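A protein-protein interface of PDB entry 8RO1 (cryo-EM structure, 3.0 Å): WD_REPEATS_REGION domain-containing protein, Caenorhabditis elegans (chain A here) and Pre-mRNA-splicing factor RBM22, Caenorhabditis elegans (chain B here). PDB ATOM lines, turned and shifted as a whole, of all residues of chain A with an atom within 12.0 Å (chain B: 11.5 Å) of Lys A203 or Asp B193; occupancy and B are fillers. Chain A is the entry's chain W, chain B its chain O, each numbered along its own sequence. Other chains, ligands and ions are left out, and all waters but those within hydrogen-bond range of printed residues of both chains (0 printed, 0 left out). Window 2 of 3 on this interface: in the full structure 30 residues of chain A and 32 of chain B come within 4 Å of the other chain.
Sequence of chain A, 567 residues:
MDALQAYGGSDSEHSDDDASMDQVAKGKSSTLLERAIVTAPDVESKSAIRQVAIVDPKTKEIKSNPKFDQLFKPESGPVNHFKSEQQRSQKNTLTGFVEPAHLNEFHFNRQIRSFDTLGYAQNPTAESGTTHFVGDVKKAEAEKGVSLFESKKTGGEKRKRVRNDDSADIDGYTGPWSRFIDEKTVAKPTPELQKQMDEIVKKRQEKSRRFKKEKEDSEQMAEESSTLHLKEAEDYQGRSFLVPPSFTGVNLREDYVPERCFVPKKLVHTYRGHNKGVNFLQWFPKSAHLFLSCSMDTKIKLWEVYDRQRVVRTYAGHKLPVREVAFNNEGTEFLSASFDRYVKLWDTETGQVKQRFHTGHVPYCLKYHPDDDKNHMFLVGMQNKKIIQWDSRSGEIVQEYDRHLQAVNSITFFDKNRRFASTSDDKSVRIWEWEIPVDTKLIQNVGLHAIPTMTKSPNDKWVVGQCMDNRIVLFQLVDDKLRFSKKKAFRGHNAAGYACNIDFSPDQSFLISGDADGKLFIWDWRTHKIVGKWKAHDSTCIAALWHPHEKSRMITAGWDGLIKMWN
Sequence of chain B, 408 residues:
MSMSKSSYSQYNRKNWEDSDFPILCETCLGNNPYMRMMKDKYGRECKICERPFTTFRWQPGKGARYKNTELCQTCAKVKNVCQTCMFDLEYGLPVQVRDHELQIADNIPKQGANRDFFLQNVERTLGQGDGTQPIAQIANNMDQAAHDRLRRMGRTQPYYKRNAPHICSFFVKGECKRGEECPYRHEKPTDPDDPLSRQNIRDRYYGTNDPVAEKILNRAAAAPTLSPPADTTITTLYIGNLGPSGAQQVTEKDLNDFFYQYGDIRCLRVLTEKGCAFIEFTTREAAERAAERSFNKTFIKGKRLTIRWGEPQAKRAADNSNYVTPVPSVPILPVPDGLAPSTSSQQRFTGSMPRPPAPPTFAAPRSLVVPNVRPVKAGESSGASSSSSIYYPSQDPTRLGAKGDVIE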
ATOM      1  N   GLN A 194     -24.064 -22.490 -14.195  1.00  0.00           N
ATOM      2  CA  GLN A 194     -24.183 -23.511 -15.233  1.00  0.00           C
ATOM      3  C   GLN A 194     -23.292 -23.194 -16.429  1.00  0.00           C
ATOM      4  O   GLN A 194     -22.545 -24.057 -16.901  1.00  0.00           O
ATOM      5  CB  GLN A 194     -25.635 -23.621 -15.699  1.00  0.00           C
ATOM      6  CG  GLN A 194     -26.604 -24.214 -14.708  1.00  0.00           C
ATOM      7  CD  GLN A 194     -27.987 -24.395 -15.302  1.00  0.00           C
ATOM      8  OE1 GLN A 194     -28.158 -24.400 -16.523  1.00  0.00           O
ATOM      9  NE2 GLN A 194     -28.990 -24.515 -14.439  1.00  0.00           N
ATOM     10  N   LYS A 195     -23.330 -21.942 -16.906  1.00  0.00           N
ATOM     11  CA  LYS A 195     -22.624 -21.596 -18.140  1.00  0.00           C
ATOM     12  C   LYS A 195     -21.115 -21.713 -17.990  1.00  0.00           C
ATOM     13  O   LYS A 195     -20.419 -22.022 -18.964  1.00  0.00           O
ATOM     14  CB  LYS A 195     -22.992 -20.185 -18.617  1.00  0.00           C
ATOM     15  CG  LYS A 195     -24.392 -20.048 -19.227  1.00  0.00           C
ATOM     16  CD  LYS A 195     -24.714 -18.601 -19.609  1.00  0.00           C
ATOM     17  CE  LYS A 195     -26.071 -18.492 -20.297  1.00  0.00           C
ATOM     18  NZ  LYS A 195     -26.394 -17.097 -20.731  1.00  0.00           N
ATOM     19  N   GLN A 196     -20.597 -21.497 -16.786  1.00  0.00           N
ATOM     20  CA  GLN A 196     -19.191 -21.773 -16.529  1.00  0.00           C
ATOM     21  C   GLN A 196     -18.898 -23.264 -16.615  1.00  0.00           C
ATOM     22  O   GLN A 196     -17.970 -23.693 -17.308  1.00  0.00           O
ATOM     23  CB  GLN A 196     -18.818 -21.251 -15.142  1.00  0.00           C
ATOM     24  CG  GLN A 196     -18.923 -19.746 -14.981  1.00  0.00           C
ATOM     25  CD  GLN A 196     -18.647 -19.296 -13.560  1.00  0.00           C
ATOM     26  OE1 GLN A 196     -18.016 -20.009 -12.784  1.00  0.00           O
ATOM     27  NE2 GLN A 196     -19.127 -18.110 -13.210  1.00  0.00           N
ATOM     28  N   MET A 197     -19.684 -24.067 -15.909  1.00  0.00           N
ATOM     29  CA  MET A 197     -19.554 -25.518 -15.982  1.00  0.00           C
ATOM     30  C   MET A 197     -19.937 -26.101 -17.343  1.00  0.00           C
ATOM     31  O   MET A 197     -19.395 -27.143 -17.729  1.00  0.00           O
ATOM     32  CB  MET A 197     -20.392 -26.131 -14.864  1.00  0.00           C
ATOM     33  CG  MET A 197     -19.580 -26.327 -13.604  1.00  0.00           C
ATOM     34  SD  MET A 197     -20.519 -27.064 -12.273  1.00  0.00           S
ATOM     35  CE  MET A 197     -21.400 -25.646 -11.640  1.00  0.00           C
ATOM     36  N   ASP A 198     -20.868 -25.473 -18.068  1.00  0.00           N
ATOM     37  CA  ASP A 198     -21.279 -25.994 -19.374  1.00  0.00           C
ATOM     38  C   ASP A 198     -20.117 -26.078 -20.358  1.00  0.00           C
ATOM     39  O   ASP A 198     -20.023 -27.036 -21.132  1.00  0.00           O
ATOM     40  CB  ASP A 198     -22.403 -25.137 -19.961  1.00  0.00           C
ATOM     41  CG  ASP A 198     -23.745 -25.364 -19.273  1.00  0.00           C
ATOM     42  OD1 ASP A 198     -23.875 -26.328 -18.489  1.00  0.00           O
ATOM     43  OD2 ASP A 198     -24.680 -24.578 -19.530  1.00  0.00           O
ATOM     44  N   GLU A 199     -19.244 -25.073 -20.373  1.00  0.00           N
ATOM     45  CA  GLU A 199     -18.091 -25.114 -21.268  1.00  0.00           C
ATOM     46  C   GLU A 199     -17.071 -26.171 -20.854  1.00  0.00           C
ATOM     47  O   GLU A 199     -16.397 -26.747 -21.715  1.00  0.00           O
ATOM     48  CB  GLU A 199     -17.444 -23.725 -21.350  1.00  0.00           C
ATOM     49  CG  GLU A 199     -16.837 -23.167 -20.053  1.00  0.00           C
ATOM     50  CD  GLU A 199     -15.770 -22.126 -20.305  1.00  0.00           C
ATOM     51  OE1 GLU A 199     -16.130 -20.963 -20.587  1.00  0.00           O
ATOM     52  OE2 GLU A 199     -14.572 -22.468 -20.215  1.00  0.00           O
ATOM     53  N   ILE A 200     -16.949 -26.426 -19.551  1.00  0.00           N
ATOM     54  CA  ILE A 200     -15.962 -27.375 -19.035  1.00  0.00           C
ATOM     55  C   ILE A 200     -16.161 -28.775 -19.614  1.00  0.00           C
ATOM     56  O   ILE A 200     -15.197 -29.415 -20.049  1.00  0.00           O
ATOM     57  CB  ILE A 200     -15.979 -27.359 -17.491  1.00  0.00           C
ATOM     58  CG1 ILE A 200     -15.299 -26.070 -17.001  1.00  0.00           C
ATOM     59  CG2 ILE A 200     -15.371 -28.647 -16.871  1.00  0.00           C
ATOM     60  CD1 ILE A 200     -15.430 -25.771 -15.521  1.00  0.00           C
ATOM     61  N   VAL A 201     -17.399 -29.275 -19.636  1.00  0.00           N
ATOM     62  CA  VAL A 201     -17.602 -30.615 -20.190  1.00  0.00           C
ATOM     63  C   VAL A 201     -17.307 -30.650 -21.685  1.00  0.00           C
ATOM     64  O   VAL A 201     -16.842 -31.673 -22.202  1.00  0.00           O
ATOM     65  CB  VAL A 201     -19.024 -31.136 -19.887  1.00  0.00           C
ATOM     66  CG1 VAL A 201     -19.218 -31.345 -18.378  1.00  0.00           C
ATOM     67  CG2 VAL A 201     -20.116 -30.245 -20.498  1.00  0.00           C
ATOM     68  N   LYS A 202     -17.567 -29.560 -22.409  1.00  0.00           N
ATOM     69  CA  LYS A 202     -17.269 -29.558 -23.838  1.00  0.00           C
ATOM     70  C   LYS A 202     -15.764 -29.558 -24.081  1.00  0.00           C
ATOM     71  O   LYS A 202     -15.273 -30.247 -24.983  1.00  0.00           O
ATOM     72  CB  LYS A 202     -17.928 -28.355 -24.513  1.00  0.00           C
ATOM     73  CG  LYS A 202     -19.436 -28.489 -24.690  1.00  0.00           C
ATOM     74  CD  LYS A 202     -20.040 -27.255 -25.344  1.00  0.00           C
ATOM     75  CE  LYS A 202     -21.542 -27.412 -25.553  1.00  0.00           C
ATOM     76  NZ  LYS A 202     -22.157 -26.226 -26.218  1.00  0.00           N
ATOM     77  N   LYS A 203     -15.018 -28.790 -23.280  1.00  0.00           N
ATOM     78  CA  LYS A 203     -13.563 -28.757 -23.391  1.00  0.00           C
ATOM     79  C   LYS A 203     -12.936 -30.116 -23.124  1.00  0.00           C
ATOM     80  O   LYS A 203     -11.907 -30.457 -23.717  1.00  0.00           O
ATOM     81  CB  LYS A 203     -12.993 -27.719 -22.429  1.00  0.00           C
ATOM     82  CG  LYS A 203     -13.108 -26.314 -22.954  1.00  0.00           C
ATOM     83  CD  LYS A 203     -12.622 -25.292 -21.956  1.00  0.00           C
ATOM     84  CE  LYS A 203     -12.480 -23.936 -22.618  1.00  0.00           C
ATOM     85  NZ  LYS A 203     -12.075 -22.882 -21.655  1.00  0.00           N
ATOM     86  N   ARG A 204     -13.541 -30.900 -22.236  1.00  0.00           N
ATOM     87  CA  ARG A 204     -13.101 -32.272 -22.027  1.00  0.00           C
ATOM     88  C   ARG A 204     -13.386 -33.151 -23.238  1.00  0.00           C
ATOM     89  O   ARG A 204     -12.604 -34.061 -23.537  1.00  0.00           O
ATOM     90  CB  ARG A 204     -13.779 -32.824 -20.778  1.00  0.00           C
ATOM     91  CG  ARG A 204     -13.323 -32.135 -19.502  1.00  0.00           C
ATOM     92  CD  ARG A 204     -14.080 -32.643 -18.294  1.00  0.00           C
ATOM     93  NE  ARG A 204     -13.633 -32.010 -17.058  1.00  0.00           N
ATOM     94  CZ  ARG A 204     -14.274 -32.066 -15.897  1.00  0.00           C
ATOM     95  NH1 ARG A 204     -13.767 -31.429 -14.846  1.00  0.00           N
ATOM     96  NH2 ARG A 204     -15.404 -32.741 -15.753  1.00  0.00           N
ATOM     97  N   GLN A 205     -14.486 -32.894 -23.950  1.00  0.00           N
ATOM     98  CA  GLN A 205     -14.831 -33.712 -25.107  1.00  0.00           C
ATOM     99  C   GLN A 205     -14.041 -33.314 -26.348  1.00  0.00           C
ATOM    100  O   GLN A 205     -13.794 -34.162 -27.213  1.00  0.00           O
ATOM    101  CB  GLN A 205     -16.331 -33.622 -25.390  1.00  0.00           C
ATOM    102  CG  GLN A 205     -17.198 -34.409 -24.413  1.00  0.00           C
ATOM    103  CD  GLN A 205     -17.070 -35.916 -24.592  1.00  0.00           C
ATOM    104  OE1 GLN A 205     -16.793 -36.401 -25.691  1.00  0.00           O
ATOM    105  NE2 GLN A 205     -17.270 -36.662 -23.509  1.00  0.00           N
ATOM    106  N   GLU A 206     -13.654 -32.040 -26.466  1.00  0.00           N
ATOM    107  CA  GLU A 206     -12.823 -31.613 -27.588  1.00  0.00           C
ATOM    108  C   GLU A 206     -11.475 -32.327 -27.645  1.00  0.00           C
ATOM    109  O   GLU A 206     -10.859 -32.359 -28.717  1.00  0.00           O
ATOM    110  CB  GLU A 206     -12.583 -30.105 -27.530  1.00  0.00           C
ATOM    111  CG  GLU A 206     -13.742 -29.262 -28.030  1.00  0.00           C
ATOM    112  CD  GLU A 206     -13.498 -27.777 -27.848  1.00  0.00           C
ATOM    113  OE1 GLU A 206     -12.320 -27.373 -27.757  1.00  0.00           O
ATOM    114  OE2 GLU A 206     -14.483 -27.011 -27.811  1.00  0.00           O
ATOM    115  N   LYS A 207     -10.991 -32.877 -26.526  1.00  0.00           N
ATOM    116  CA  LYS A 207      -9.743 -33.636 -26.554  1.00  0.00           C
ATOM    117  C   LYS A 207      -9.810 -34.837 -27.489  1.00  0.00           C
ATOM    118  O   LYS A 207      -8.786 -35.226 -28.064  1.00  0.00           O
ATOM    119  CB  LYS A 207      -9.380 -34.109 -25.148  1.00  0.00           C
ATOM    120  CG  LYS A 207      -8.938 -33.012 -24.205  1.00  0.00           C
ATOM    121  CD  LYS A 207      -8.440 -33.613 -22.903  1.00  0.00           C
ATOM    122  CE  LYS A 207      -7.977 -32.553 -21.923  1.00  0.00           C
ATOM    123  NZ  LYS A 207      -7.520 -33.169 -20.647  1.00  0.00           N
ATOM    124  N   SER A 208     -10.987 -35.439 -27.651  1.00  0.00           N
ATOM    125  CA  SER A 208     -11.139 -36.640 -28.473  1.00  0.00           C
ATOM    126  C   SER A 208     -10.751 -36.395 -29.931  1.00  0.00           C
ATOM    127  O   SER A 208     -10.552 -35.255 -30.350  1.00  0.00           O
ATOM    128  CB  SER A 208     -12.578 -37.157 -28.399  1.00  0.00           C
ATOM    129  OG  SER A 208     -12.966 -37.393 -27.055  1.00  0.00           O
ATOM    130  N   VAL B 172     -21.865 -31.270 -10.695  1.00  0.00           N
ATOM    131  CA  VAL B 172     -21.278 -30.655 -11.882  1.00  0.00           C
ATOM    132  C   VAL B 172     -22.268 -30.690 -13.042  1.00  0.00           C
ATOM    133  O   VAL B 172     -22.477 -29.680 -13.715  1.00  0.00           O
ATOM    134  CB  VAL B 172     -19.939 -31.337 -12.233  1.00  0.00           C
ATOM    135  CG1 VAL B 172     -19.326 -30.790 -13.534  1.00  0.00           C
ATOM    136  CG2 VAL B 172     -18.941 -31.097 -11.109  1.00  0.00           C
ATOM    137  N   LYS B 188     -17.064 -25.299  -7.578  1.00  0.00           N
ATOM    138  CA  LYS B 188     -16.460 -25.295  -8.907  1.00  0.00           C
ATOM    139  C   LYS B 188     -15.335 -26.333  -9.020  1.00  0.00           C
ATOM    140  O   LYS B 188     -14.410 -26.319  -8.198  1.00  0.00           O
ATOM    141  CB  LYS B 188     -15.891 -23.903  -9.198  1.00  0.00           C
ATOM    142  CG  LYS B 188     -16.737 -23.033 -10.145  1.00  0.00           C
ATOM    143  CD  LYS B 188     -16.903 -23.507 -11.601  1.00  0.00           C
ATOM    144  CE  LYS B 188     -15.603 -23.887 -12.312  1.00  0.00           C
ATOM    145  NZ  LYS B 188     -14.706 -22.722 -12.552  1.00  0.00           N
ATOM    146  N   PRO B 189     -15.356 -27.221 -10.020  1.00  0.00           N
ATOM    147  CA  PRO B 189     -14.172 -28.041 -10.293  1.00  0.00           C
ATOM    148  C   PRO B 189     -13.050 -27.213 -10.902  1.00  0.00           C
ATOM    149  O   PRO B 189     -13.211 -26.040 -11.243  1.00  0.00           O
ATOM    150  CB  PRO B 189     -14.683 -29.111 -11.261  1.00  0.00           C
ATOM    151  CG  PRO B 189     -15.776 -28.476 -11.962  1.00  0.00           C
ATOM    152  CD  PRO B 189     -16.434 -27.553 -10.974  1.00  0.00           C
ATOM    153  N   THR B 190     -11.881 -27.838 -11.010  1.00  0.00           N
ATOM    154  CA  THR B 190     -10.765 -27.242 -11.738  1.00  0.00           C
ATOM    155  C   THR B 190     -10.987 -27.281 -13.242  1.00  0.00           C
ATOM    156  O   THR B 190     -11.394 -28.304 -13.801  1.00  0.00           O
ATOM    157  CB  THR B 190      -9.467 -27.974 -11.390  1.00  0.00           C
ATOM    158  OG1 THR B 190      -9.216 -27.846  -9.988  1.00  0.00           O
ATOM    159  CG2 THR B 190      -8.248 -27.432 -12.189  1.00  0.00           C
ATOM    160  N   ASP B 191     -10.713 -26.151 -13.895  1.00  0.00           N
ATOM    161  CA  ASP B 191     -10.997 -26.004 -15.310  1.00  0.00           C
ATOM    162  C   ASP B 191     -10.091 -26.932 -16.126  1.00  0.00           C
ATOM    163  O   ASP B 191      -8.937 -27.155 -15.758  1.00  0.00           O
ATOM    164  CB  ASP B 191     -10.784 -24.563 -15.749  1.00  0.00           C
ATOM    165  CG  ASP B 191     -11.668 -23.591 -14.996  1.00  0.00           C
ATOM    166  OD1 ASP B 191     -12.561 -24.051 -14.253  1.00  0.00           O
ATOM    167  OD2 ASP B 191     -11.479 -22.365 -15.153  1.00  0.00           O
ATOM    168  N   PRO B 192     -10.576 -27.475 -17.250  1.00  0.00           N
ATOM    169  CA  PRO B 192      -9.773 -28.468 -17.983  1.00  0.00           C
ATOM    170  C   PRO B 192      -8.588 -27.872 -18.728  1.00  0.00           C
ATOM    171  O   PRO B 192      -7.709 -28.632 -19.157  1.00  0.00           O
ATOM    172  CB  PRO B 192     -10.779 -29.078 -18.966  1.00  0.00           C
ATOM    173  CG  PRO B 192     -11.769 -28.011 -19.187  1.00  0.00           C
ATOM    174  CD  PRO B 192     -11.886 -27.277 -17.889  1.00  0.00           C
ATOM    175  N   ASP B 193      -8.538 -26.551 -18.899  1.00  0.00           N
ATOM    176  CA  ASP B 193      -7.341 -25.899 -19.426  1.00  0.00           C
ATOM    177  C   ASP B 193      -6.188 -25.900 -18.431  1.00  0.00           C
ATOM    178  O   ASP B 193      -5.026 -25.928 -18.841  1.00  0.00           O
ATOM    179  CB  ASP B 193      -7.671 -24.459 -19.817  1.00  0.00           C
ATOM    180  CG  ASP B 193      -8.747 -24.374 -20.878  1.00  0.00           C
ATOM    181  OD1 ASP B 193      -8.665 -25.129 -21.868  1.00  0.00           O
ATOM    182  OD2 ASP B 193      -9.672 -23.548 -20.725  1.00  0.00           O
ATOM    183  N   ASP B 194      -6.489 -25.897 -17.142  1.00  0.00           N
ATOM    184  CA  ASP B 194      -5.562 -25.799 -16.020  1.00  0.00           C
ATOM    185  C   ASP B 194      -4.672 -27.041 -15.880  1.00  0.00           C
ATOM    186  O   ASP B 194      -5.089 -27.989 -15.201  1.00  0.00           O
ATOM    187  CB  ASP B 194      -6.339 -25.535 -14.727  1.00  0.00           C
ATOM    188  CG  ASP B 194      -5.467 -24.947 -13.635  1.00  0.00           C
ATOM    189  OD1 ASP B 194      -4.230 -24.911 -13.810  1.00  0.00           O
ATOM    190  OD2 ASP B 194      -6.015 -24.510 -12.602  1.00  0.00           O
ATOM    191  N   PRO B 195      -3.500 -27.118 -16.560  1.00  0.00           N
ATOM    192  CA  PRO B 195      -2.696 -28.370 -16.589  1.00  0.00           C
ATOM    193  C   PRO B 195      -2.458 -29.054 -15.246  1.00  0.00           C
ATOM    194  O   PRO B 195      -2.232 -30.271 -15.212  1.00  0.00           O
ATOM    195  CB  PRO B 195      -1.358 -27.913 -17.187  1.00  0.00           C
ATOM    196  CG  PRO B 195      -1.261 -26.496 -16.837  1.00  0.00           C
ATOM    197  CD  PRO B 195      -2.649 -25.975 -16.951  1.00  0.00           C
ATOM    198  N   LEU B 196      -2.479 -28.297 -14.146  1.00  0.00           N
ATOM    199  CA  LEU B 196      -2.446 -28.865 -12.801  1.00  0.00           C
ATOM    200  C   LEU B 196      -3.520 -29.929 -12.574  1.00  0.00           C
ATOM    201  O   LEU B 196      -3.335 -30.822 -11.744  1.00  0.00           O
ATOM    202  CB  LEU B 196      -2.619 -27.752 -11.764  1.00  0.00           C
ATOM    203  CG  LEU B 196      -1.569 -26.645 -11.669  1.00  0.00           C
ATOM    204  CD1 LEU B 196      -2.003 -25.610 -10.650  1.00  0.00           C
ATOM    205  CD2 LEU B 196      -0.205 -27.191 -11.300  1.00  0.00           C
ATOM    206  N   SER B 197      -4.659 -29.830 -13.257  1.00  0.00           N
ATOM    207  CA  SER B 197      -5.653 -30.902 -13.217  1.00  0.00           C
ATOM    208  C   SER B 197      -5.155 -32.228 -13.797  1.00  0.00           C
ATOM    209  O   SER B 197      -5.616 -33.292 -13.371  1.00  0.00           O
ATOM    210  CB  SER B 197      -6.899 -30.458 -13.976  1.00  0.00           C
ATOM    211  OG  SER B 197      -6.623 -30.355 -15.358  1.00  0.00           O
ATOM    212  N   ARG B 198      -4.250 -32.198 -14.775  1.00  0.00           N
ATOM    213  CA  ARG B 198      -3.979 -33.394 -15.578  1.00  0.00           C
ATOM    214  C   ARG B 198      -3.184 -34.487 -14.851  1.00  0.00           C
ATOM    215  O   ARG B 198      -3.355 -35.664 -15.188  1.00  0.00           O
ATOM    216  CB  ARG B 198      -3.286 -32.991 -16.877  1.00  0.00           C
ATOM    217  CG  ARG B 198      -4.154 -32.065 -17.714  1.00  0.00           C
ATOM    218  CD  ARG B 198      -3.562 -31.735 -19.059  1.00  0.00           C
ATOM    219  NE  ARG B 198      -4.431 -30.801 -19.769  1.00  0.00           N
ATOM    220  CZ  ARG B 198      -4.262 -30.395 -21.021  1.00  0.00           C
ATOM    221  NH1 ARG B 198      -5.136 -29.541 -21.545  1.00  0.00           N
ATOM    222  NH2 ARG B 198      -3.249 -30.814 -21.763  1.00  0.00           N
ATOM    223  N   GLN B 199      -2.312 -34.122 -13.898  1.00  0.00           N
ATOM    224  CA  GLN B 199      -1.270 -34.966 -13.263  1.00  0.00           C
ATOM    225  C   GLN B 199      -1.685 -36.420 -13.033  1.00  0.00           C
ATOM    226  O   GLN B 199      -2.681 -36.696 -12.362  1.00  0.00           O
ATOM    227  CB  GLN B 199      -0.787 -34.363 -11.911  1.00  0.00           C
ATOM    228  CG  GLN B 199      -1.289 -32.975 -11.458  1.00  0.00           C
ATOM    229  CD  GLN B 199      -0.814 -32.560 -10.092  1.00  0.00           C
ATOM    230  OE1 GLN B 199      -1.612 -32.243  -9.220  1.00  0.00           O
ATOM    231  NE2 GLN B 199       0.491 -32.584  -9.888  1.00  0.00           N
ATOM    232  N   PRO B 211       3.019 -31.270 -13.192  1.00  0.00           N
ATOM    233  CA  PRO B 211       2.674 -29.838 -13.315  1.00  0.00           C
ATOM    234  C   PRO B 211       2.908 -28.996 -12.076  1.00  0.00           C
ATOM    235  O   PRO B 211       3.385 -27.861 -12.181  1.00  0.00           O
ATOM    236  CB  PRO B 211       1.182 -29.877 -13.659  1.00  0.00           C
ATOM    237  CG  PRO B 211       0.994 -31.125 -14.344  1.00  0.00           C
ATOM    238  CD  PRO B 211       1.870 -32.093 -13.610  1.00  0.00           C
ATOM    239  N   GLU B 214       6.642 -28.169 -11.632  1.00  0.00           N
ATOM    240  CA  GLU B 214       7.105 -27.115 -12.526  1.00  0.00           C
ATOM    241  C   GLU B 214       6.685 -25.732 -12.047  1.00  0.00           C
ATOM    242  O   GLU B 214       7.464 -24.779 -12.136  1.00  0.00           O
ATOM    243  CB  GLU B 214       6.590 -27.384 -13.935  1.00  0.00           C
ATOM    244  CG  GLU B 214       7.210 -28.623 -14.553  1.00  0.00           C
ATOM    245  CD  GLU B 214       6.778 -28.846 -15.982  1.00  0.00           C
ATOM    246  OE1 GLU B 214       5.879 -28.117 -16.451  1.00  0.00           O
ATOM    247  OE2 GLU B 214       7.333 -29.753 -16.635  1.00  0.00           O
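The side-chain carboxylate (OD1) of Asp B191 lies within salt-bridge range of the side-chain amino group (NZ) of Lys B188 (3.0 Å).
The side-chain carboxylate (OE2) of Glu A199 lies within salt-bridge range of the side-chain amino group (NZ) of Lys A203 (2.9 Å).
Of the 15 printed residues of chain B, 6 touch a printed residue of chain A.
Printed residues of chain B that touch a printed residue of chain A: Val B172, Lys B188, Asp B191, Pro B192, Asp B193 and Arg B198.
Hydrophobic or aromatic side chains of chain B within 4 Å of the printed part of chain A: Pro B192.
Among the printed residues, Asp or Glu carboxylates within 4 Å of a Lys or Arg side-chain nitrogen of the other chain: Lys A203 with Asp B193 (2.7 Å).
NZ of Lys A203 is in salt-bridge range of OD2 of Asp B193, 2.7 Å away.
SD of Met A197 lies close to O of Val B172 (3.6 Å).
Of chain B, only Lys B188 (3.7 Å), Asp B191 (3.6 Å) and Pro B192 (3.7 Å) come within 4 Å of Ile A200.
No residue of chain B comes within 4 Å of Val A201.
Lys A203 touches just these residues of chain B: Pro B192 (3.5 Å) and Asp B193 (2.7 Å).
No residue of chain B comes within 4 Å of Glu A206.
Printed residues of chain A within 4 Å of Lys B188: Gln A196 (3.9 Å) and Ile A200 (3.7 Å).
Printed residues of chain A within 4 Å of Pro B192: Ile A200 and Lys A203.
Ser B197 touches none of the printed residues of chain A.
The nearest residue of chain A that does not touch Asp B193 is Glu A199 (5.0 Å).
The nearest printed residue of chain A that does not touch Pro B192 is Arg A204 (4.01 Å).
Among the printed residues, merely in contact across the chains: Lys A203 with Pro B192 (3.5 Å), Ile A200 with Asp B191 (3.6 Å), Ile A200 with Lys B188 (3.7 Å), Ile A200 with Pro B192 (3.7 Å), Gln A196 with Lys B188 (3.9 Å) and Lys A207 with Arg B198 (3.99 Å).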
